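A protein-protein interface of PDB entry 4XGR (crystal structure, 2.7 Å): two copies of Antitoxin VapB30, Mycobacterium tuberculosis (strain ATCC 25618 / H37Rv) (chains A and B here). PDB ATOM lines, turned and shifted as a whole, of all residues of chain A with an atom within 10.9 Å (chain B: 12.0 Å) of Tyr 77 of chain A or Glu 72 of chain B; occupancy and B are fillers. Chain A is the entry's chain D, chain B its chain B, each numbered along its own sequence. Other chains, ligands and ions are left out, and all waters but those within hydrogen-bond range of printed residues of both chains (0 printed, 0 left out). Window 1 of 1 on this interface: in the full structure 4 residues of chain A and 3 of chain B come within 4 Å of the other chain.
OE2 of Glu 72 of chain B sits close to O of Tyr 77 of chain A (3.4 Å).
The backbone NH of Tyr 77 of chain B sits at hydrogen-bond distance from the backbone carbonyl oxygen of Glu 72 of chain B, 3.5 Å away.
OG of Ser 70 of chain A sits at hydrogen-bond distance from N of Ala 73 of chain A, at 3.3 Å.
Among the printed residues, merely in contact across the chains: Tyr 77 of chain A with Tyr 77 of chain B, Glu 72 of chain A with Tyr 77 of chain B, Asp 78 of chain A with Glu 72 of chain B, Asp 78 of chain A with Glu 79 of chain B and Ser 70 of chain A with Glu 79 of chain B.
Printed residues of chain B within 4 Å of Ser 70 of chain A: Glu 79.
Printed residues of chain B within 4 Å of Glu 72 of chain A: Tyr 77.
Ala 73 of chain A touches none of the printed residues of chain B.
No residue of chain B comes within 4 Å of Gly 76 of chain A.
Of the printed residues of chain B, Tyr 77 of chain A touches Glu 72 (3.1 Å) and Tyr 77 (3.3 Å).
Printed residues of chain B within 4 Å of Asp 78 of chain A: Glu 72 (3.6 Å) and Glu 79 (3.8 Å).
No residue of chain B comes within 4 Å of Glu 79 of chain A.
Of chain A, only Tyr 77 and Asp 78 come within 4 Å of Glu 72 of chain B.
No residue of chain A comes within 4 Å of Ala 73 of chain B.
No residue of chain A comes within 4 Å of Gly 76 of chain B.
Printed residues of chain A within 4 Å of Glu 79 of chain B: Ser 70 and Asp 78.
Hydrophobic or aromatic side chains of chain A that line the printed part of chain B: Tyr 77.
Of the 13 printed residues of chain B, 3 touch a printed residue of chain A.
Printed residues of chain B that touch a printed residue of chain A: Glu 72, Tyr 77 and Glu 79.
Among the printed residues, no Asp or Glu carboxylate lies within 4 Å of a Lys or Arg side-chain nitrogen of the other chain.
Ser 70 of chain A touches Glu 79 of chain B, but with the chains exchanged Glu 79 of chain A does not touch Ser 70 of chain B (7.9 Å).
Tyr 77 of chain B touches its own counterpart, Tyr 77 of chain A.
Asp 78 of chain A touches Glu 72 of chain B, but with the chains exchanged Glu 72 of chain A does not touch Asp 78 of chain B (6.9 Å).
Asp 78 of chain A touches Glu 79 of chain B, but with the chains exchanged Glu 79 of chain A does not touch Asp 78 of chain B (6.5 Å).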
ATOM      1  N   ARG A  69      27.442 -18.413   1.677  1.00  0.00           N
ATOM      2  CA  ARG A  69      27.460 -19.074   0.360  1.00  0.00           C
ATOM      3  C   ARG A  69      26.093 -19.663   0.040  1.00  0.00           C
ATOM      4  O   ARG A  69      25.257 -19.836   0.931  1.00  0.00           O
ATOM      5  CB  ARG A  69      28.523 -20.188   0.310  1.00  0.00           C
ATOM      6  CG  ARG A  69      29.977 -19.717   0.386  1.00  0.00           C
ATOM      7  CD  ARG A  69      30.705 -19.719  -0.958  1.00  0.00           C
ATOM      8  NE  ARG A  69      32.168 -19.644  -0.787  1.00  0.00           N
ATOM      9  CZ  ARG A  69      32.922 -18.532  -0.786  1.00  0.00           C
ATOM     10  NH1 ARG A  69      32.397 -17.310  -0.960  1.00  0.00           N
ATOM     11  NH2 ARG A  69      34.238 -18.641  -0.605  1.00  0.00           N
ATOM     12  N   SER A  70      25.867 -19.966  -1.234  1.00  0.00           N
ATOM     13  CA  SER A  70      24.581 -20.516  -1.686  1.00  0.00           C
ATOM     14  C   SER A  70      24.340 -21.890  -1.070  1.00  0.00           C
ATOM     15  O   SER A  70      25.277 -22.696  -0.957  1.00  0.00           O
ATOM     16  CB  SER A  70      24.533 -20.639  -3.218  1.00  0.00           C
ATOM     17  OG  SER A  70      25.331 -21.725  -3.684  1.00  0.00           O
ATOM     18  N   ALA A  71      23.084 -22.135  -0.678  1.00  0.00           N
ATOM     19  CA  ALA A  71      22.606 -23.451  -0.214  1.00  0.00           C
ATOM     20  C   ALA A  71      23.230 -24.608  -0.994  1.00  0.00           C
ATOM     21  O   ALA A  71      23.813 -25.522  -0.404  1.00  0.00           O
ATOM     22  CB  ALA A  71      21.081 -23.524  -0.324  1.00  0.00           C
ATOM     23  N   GLU A  72      23.142 -24.531  -2.323  1.00  0.00           N
ATOM     24  CA  GLU A  72      23.676 -25.582  -3.189  1.00  0.00           C
ATOM     25  C   GLU A  72      25.145 -25.865  -2.808  1.00  0.00           C
ATOM     26  O   GLU A  72      25.497 -26.993  -2.462  1.00  0.00           O
ATOM     27  CB  GLU A  72      23.558 -25.246  -4.697  1.00  0.00           C
ATOM     28  CG  GLU A  72      22.284 -24.535  -5.204  1.00  0.00           C
ATOM     29  CD  GLU A  72      20.966 -25.054  -4.626  1.00  0.00           C
ATOM     30  OE1 GLU A  72      20.180 -24.236  -4.088  1.00  0.00           O
ATOM     31  OE2 GLU A  72      20.707 -26.270  -4.709  1.00  0.00           O
ATOM     32  N   ALA A  73      25.969 -24.816  -2.806  1.00  0.00           N
ATOM     33  CA  ALA A  73      27.432 -24.933  -2.615  1.00  0.00           C
ATOM     34  C   ALA A  73      27.895 -25.514  -1.265  1.00  0.00           C
ATOM     35  O   ALA A  73      28.910 -26.216  -1.208  1.00  0.00           O
ATOM     36  CB  ALA A  73      28.092 -23.578  -2.837  1.00  0.00           C
ATOM     37  N   ILE A  74      27.178 -25.210  -0.187  1.00  0.00           N
ATOM     38  CA  ILE A  74      27.553 -25.726   1.138  1.00  0.00           C
ATOM     39  C   ILE A  74      27.150 -27.190   1.338  1.00  0.00           C
ATOM     40  O   ILE A  74      27.662 -27.855   2.237  1.00  0.00           O
ATOM     41  CB  ILE A  74      27.034 -24.835   2.302  1.00  0.00           C
ATOM     42  CG1 ILE A  74      25.514 -24.676   2.274  1.00  0.00           C
ATOM     43  CG2 ILE A  74      27.707 -23.469   2.247  1.00  0.00           C
ATOM     44  CD1 ILE A  74      24.918 -24.221   3.583  1.00  0.00           C
ATOM     45  N   LEU A  75      26.253 -27.688   0.488  1.00  0.00           N
ATOM     46  CA  LEU A  75      25.922 -29.117   0.415  1.00  0.00           C
ATOM     47  C   LEU A  75      26.947 -29.915  -0.405  1.00  0.00           C
ATOM     48  O   LEU A  75      26.725 -31.101  -0.682  1.00  0.00           O
ATOM     49  CB  LEU A  75      24.534 -29.298  -0.202  1.00  0.00           C
ATOM     50  CG  LEU A  75      23.377 -28.609   0.520  1.00  0.00           C
ATOM     51  CD1 LEU A  75      22.208 -28.361  -0.420  1.00  0.00           C
ATOM     52  CD2 LEU A  75      22.929 -29.410   1.727  1.00  0.00           C
ATOM     53  N   GLY A  76      28.050 -29.272  -0.803  1.00  0.00           N
ATOM     54  CA  GLY A  76      29.183 -29.942  -1.435  1.00  0.00           C
ATOM     55  C   GLY A  76      29.099 -29.985  -2.941  1.00  0.00           C
ATOM     56  O   GLY A  76      29.912 -30.649  -3.595  1.00  0.00           O
ATOM     57  N   TYR A  77      28.133 -29.255  -3.497  1.00  0.00           N
ATOM     58  CA  TYR A  77      27.799 -29.345  -4.914  1.00  0.00           C
ATOM     59  C   TYR A  77      28.249 -28.077  -5.622  1.00  0.00           C
ATOM     60  O   TYR A  77      27.456 -27.385  -6.270  1.00  0.00           O
ATOM     61  CB  TYR A  77      26.297 -29.619  -5.094  1.00  0.00           C
ATOM     62  CG  TYR A  77      25.841 -30.965  -4.538  1.00  0.00           C
ATOM     63  CD1 TYR A  77      26.521 -32.147  -4.858  1.00  0.00           C
ATOM     64  CD2 TYR A  77      24.725 -31.066  -3.700  1.00  0.00           C
ATOM     65  CE1 TYR A  77      26.113 -33.376  -4.359  1.00  0.00           C
ATOM     66  CE2 TYR A  77      24.307 -32.298  -3.201  1.00  0.00           C
ATOM     67  CZ  TYR A  77      25.004 -33.450  -3.534  1.00  0.00           C
ATOM     68  OH  TYR A  77      24.609 -34.680  -3.049  1.00  0.00           O
ATOM     69  N   ASP A  78      29.546 -27.796  -5.489  1.00  0.00           N
ATOM     70  CA  ASP A  78      30.193 -26.679  -6.175  1.00  0.00           C
ATOM     71  C   ASP A  78      31.720 -26.848  -6.147  1.00  0.00           C
ATOM     72  O   ASP A  78      32.401 -26.330  -5.253  1.00  0.00           O
ATOM     73  CB  ASP A  78      29.766 -25.338  -5.549  1.00  0.00           C
ATOM     74  CG  ASP A  78      30.043 -24.141  -6.452  1.00  0.00           C
ATOM     75  OD1 ASP A  78      30.259 -24.323  -7.671  1.00  0.00           O
ATOM     76  OD2 ASP A  78      30.026 -23.003  -5.936  1.00  0.00           O
ATOM     77  N   GLU A  79      32.235 -27.652  -7.075  1.00  0.00           N
ATOM     78  CA  GLU A  79      33.660 -27.829  -7.273  1.00  0.00           C
ATOM     79  C   GLU A  79      33.926 -27.605  -8.750  1.00  0.00           C
ATOM     80  O   GLU A  79      33.007 -27.365  -9.524  1.00  0.00           O
ATOM     81  CB  GLU A  79      34.129 -29.213  -6.853  1.00  0.00           C
ATOM     82  CG  GLU A  79      33.668 -30.341  -7.768  1.00  0.00           C
ATOM     83  CD  GLU A  79      34.696 -30.849  -8.814  1.00  0.00           C
ATOM     84  OE1 GLU A  79      35.923 -30.671  -8.649  1.00  0.00           O
ATOM     85  OE2 GLU A  79      34.271 -31.480  -9.810  1.00  0.00           O
ATOM     86  N   ASP B  67      22.592 -39.039 -22.098  1.00  0.00           N
ATOM     87  CA  ASP B  67      22.972 -37.845 -21.346  1.00  0.00           C
ATOM     88  C   ASP B  67      24.460 -37.909 -20.961  1.00  0.00           C
ATOM     89  O   ASP B  67      24.851 -38.706 -20.093  1.00  0.00           O
ATOM     90  CB  ASP B  67      22.085 -37.735 -20.106  1.00  0.00           C
ATOM     91  CG  ASP B  67      22.260 -36.432 -19.375  1.00  0.00           C
ATOM     92  OD1 ASP B  67      23.391 -36.188 -18.908  1.00  0.00           O
ATOM     93  OD2 ASP B  67      21.269 -35.674 -19.246  1.00  0.00           O
ATOM     94  N   ASN B  68      25.272 -37.069 -21.615  1.00  0.00           N
ATOM     95  CA  ASN B  68      26.700 -36.910 -21.290  1.00  0.00           C
ATOM     96  C   ASN B  68      26.942 -35.809 -20.244  1.00  0.00           C
ATOM     97  O   ASN B  68      28.073 -35.605 -19.812  1.00  0.00           O
ATOM     98  CB  ASN B  68      27.516 -36.630 -22.567  1.00  0.00           C
ATOM     99  CG  ASN B  68      28.912 -37.255 -22.534  1.00  0.00           C
ATOM    100  OD1 ASN B  68      29.589 -37.270 -21.506  1.00  0.00           O
ATOM    101  ND2 ASN B  68      29.347 -37.768 -23.674  1.00  0.00           N
ATOM    102  N   ARG B  69      25.880 -35.089 -19.867  1.00  0.00           N
ATOM    103  CA  ARG B  69      25.885 -34.210 -18.684  1.00  0.00           C
ATOM    104  C   ARG B  69      26.330 -35.200 -17.597  1.00  0.00           C
ATOM    105  O   ARG B  69      25.620 -36.160 -17.294  1.00  0.00           O
ATOM    106  CB  ARG B  69      24.482 -33.598 -18.451  1.00  0.00           C
ATOM    107  CG  ARG B  69      24.422 -32.109 -18.180  1.00  0.00           C
ATOM    108  CD  ARG B  69      23.203 -31.732 -17.329  1.00  0.00           C
ATOM    109  NE  ARG B  69      21.884 -32.079 -17.871  1.00  0.00           N
ATOM    110  CZ  ARG B  69      21.116 -33.112 -17.500  1.00  0.00           C
ATOM    111  NH1 ARG B  69      21.513 -34.001 -16.599  1.00  0.00           N
ATOM    112  NH2 ARG B  69      19.928 -33.282 -18.077  1.00  0.00           N
ATOM    113  N   SER B  70      27.519 -34.981 -17.050  1.00  0.00           N
ATOM    114  CA  SER B  70      28.206 -35.997 -16.265  1.00  0.00           C
ATOM    115  C   SER B  70      28.170 -35.658 -14.769  1.00  0.00           C
ATOM    116  O   SER B  70      28.530 -34.552 -14.353  1.00  0.00           O
ATOM    117  CB  SER B  70      29.647 -36.234 -16.722  1.00  0.00           C
ATOM    118  OG  SER B  70      29.670 -36.827 -18.013  1.00  0.00           O
ATOM    119  N   ALA B  71      27.691 -36.626 -13.984  1.00  0.00           N
ATOM    120  CA  ALA B  71      27.888 -36.704 -12.531  1.00  0.00           C
ATOM    121  C   ALA B  71      26.967 -35.824 -11.672  1.00  0.00           C
ATOM    122  O   ALA B  71      26.102 -36.358 -10.977  1.00  0.00           O
ATOM    123  CB  ALA B  71      29.365 -36.491 -12.169  1.00  0.00           C
ATOM    124  N   GLU B  72      27.155 -34.500 -11.707  1.00  0.00           N
ATOM    125  CA  GLU B  72      26.526 -33.575 -10.730  1.00  0.00           C
ATOM    126  C   GLU B  72      25.429 -32.666 -11.288  1.00  0.00           C
ATOM    127  O   GLU B  72      24.572 -32.199 -10.539  1.00  0.00           O
ATOM    128  CB  GLU B  72      27.604 -32.709 -10.077  1.00  0.00           C
ATOM    129  CG  GLU B  72      27.119 -31.899  -8.884  1.00  0.00           C
ATOM    130  CD  GLU B  72      28.259 -31.369  -8.040  1.00  0.00           C
ATOM    131  OE1 GLU B  72      29.000 -32.193  -7.449  1.00  0.00           O
ATOM    132  OE2 GLU B  72      28.412 -30.130  -7.969  1.00  0.00           O
ATOM    133  N   ALA B  73      25.469 -32.386 -12.585  1.00  0.00           N
ATOM    134  CA  ALA B  73      24.400 -31.626 -13.236  1.00  0.00           C
ATOM    135  C   ALA B  73      23.073 -32.401 -13.344  1.00  0.00           C
ATOM    136  O   ALA B  73      21.985 -31.794 -13.358  1.00  0.00           O
ATOM    137  CB  ALA B  73      24.861 -31.175 -14.601  1.00  0.00           C
ATOM    138  N   ILE B  74      23.157 -33.698 -13.271  1.00  0.00           N
ATOM    139  CA  ILE B  74      21.970 -34.506 -13.320  1.00  0.00           C
ATOM    140  C   ILE B  74      21.152 -34.259 -12.084  1.00  0.00           C
ATOM    141  O   ILE B  74      19.958 -34.240 -12.098  1.00  0.00           O
ATOM    142  CB  ILE B  74      22.361 -35.964 -13.463  1.00  0.00           C
ATOM    143  CG1 ILE B  74      23.142 -36.112 -14.722  1.00  0.00           C
ATOM    144  CG2 ILE B  74      21.172 -36.843 -13.483  1.00  0.00           C
ATOM    145  CD1 ILE B  74      23.577 -37.504 -14.993  1.00  0.00           C
ATOM    146  N   LEU B  75      21.836 -34.041 -11.003  1.00  0.00           N
ATOM    147  CA  LEU B  75      21.193 -33.754  -9.725  1.00  0.00           C
ATOM    148  C   LEU B  75      20.556 -32.353  -9.631  1.00  0.00           C
ATOM    149  O   LEU B  75      20.076 -31.958  -8.554  1.00  0.00           O
ATOM    150  CB  LEU B  75      22.218 -33.938  -8.602  1.00  0.00           C
ATOM    151  CG  LEU B  75      22.980 -35.277  -8.601  1.00  0.00           C
ATOM    152  CD1 LEU B  75      23.710 -35.457  -7.274  1.00  0.00           C
ATOM    153  CD2 LEU B  75      22.064 -36.467  -8.883  1.00  0.00           C
ATOM    154  N   GLY B  76      20.530 -31.618 -10.745  1.00  0.00           N
ATOM    155  CA  GLY B  76      20.121 -30.213 -10.762  1.00  0.00           C
ATOM    156  C   GLY B  76      21.059 -29.256 -10.034  1.00  0.00           C
ATOM    157  O   GLY B  76      20.616 -28.213  -9.577  1.00  0.00           O
ATOM    158  N   TYR B  77      22.355 -29.587  -9.963  1.00  0.00           N
ATOM    159  CA  TYR B  77      23.321 -28.862  -9.109  1.00  0.00           C
ATOM    160  C   TYR B  77      24.532 -28.290  -9.853  1.00  0.00           C
ATOM    161  O   TYR B  77      25.656 -28.335  -9.331  1.00  0.00           O
ATOM    162  CB  TYR B  77      23.837 -29.764  -7.968  1.00  0.00           C
ATOM    163  CG  TYR B  77      22.840 -30.141  -6.890  1.00  0.00           C
ATOM    164  CD1 TYR B  77      21.984 -29.193  -6.317  1.00  0.00           C
ATOM    165  CD2 TYR B  77      22.789 -31.449  -6.397  1.00  0.00           C
ATOM    166  CE1 TYR B  77      21.085 -29.552  -5.314  1.00  0.00           C
ATOM    167  CE2 TYR B  77      21.894 -31.814  -5.393  1.00  0.00           C
ATOM    168  CZ  TYR B  77      21.049 -30.866  -4.856  1.00  0.00           C
ATOM    169  OH  TYR B  77      20.181 -31.241  -3.869  1.00  0.00           O
ATOM    170  N   ASP B  78      24.320 -27.744 -11.050  1.00  0.00           N
ATOM    171  CA  ASP B  78      25.374 -26.965 -11.716  1.00  0.00           C
ATOM    172  C   ASP B  78      25.126 -25.446 -11.693  1.00  0.00           C
ATOM    173  O   ASP B  78      26.038 -24.683 -12.010  1.00  0.00           O
ATOM    174  CB  ASP B  78      25.606 -27.462 -13.152  1.00  0.00           C
ATOM    175  CG  ASP B  78      27.026 -27.175 -13.646  1.00  0.00           C
ATOM    176  OD1 ASP B  78      27.265 -26.069 -14.174  1.00  0.00           O
ATOM    177  OD2 ASP B  78      27.906 -28.050 -13.501  1.00  0.00           O
ATOM    178  N   GLU B  79      23.920 -25.018 -11.290  1.00  0.00           N
ATOM    179  CA  GLU B  79      23.525 -23.590 -11.213  1.00  0.00           C
ATOM    180  C   GLU B  79      23.962 -22.740 -12.410  1.00  0.00           C
ATOM    181  O   GLU B  79      23.182 -21.947 -12.930  1.00  0.00           O
ATOM    182  CB  GLU B  79      23.968 -22.933  -9.882  1.00  0.00           C
ATOM    183  CG  GLU B  79      25.476 -22.813  -9.624  1.00  0.00           C
ATOM    184  CD  GLU B  79      25.821 -22.080  -8.327  1.00  0.00           C
ATOM    185  OE1 GLU B  79      27.022 -22.036  -7.980  1.00  0.00           O
ATOM    186  OE2 GLU B  79      24.912 -21.551  -7.643  1.00  0.00           O
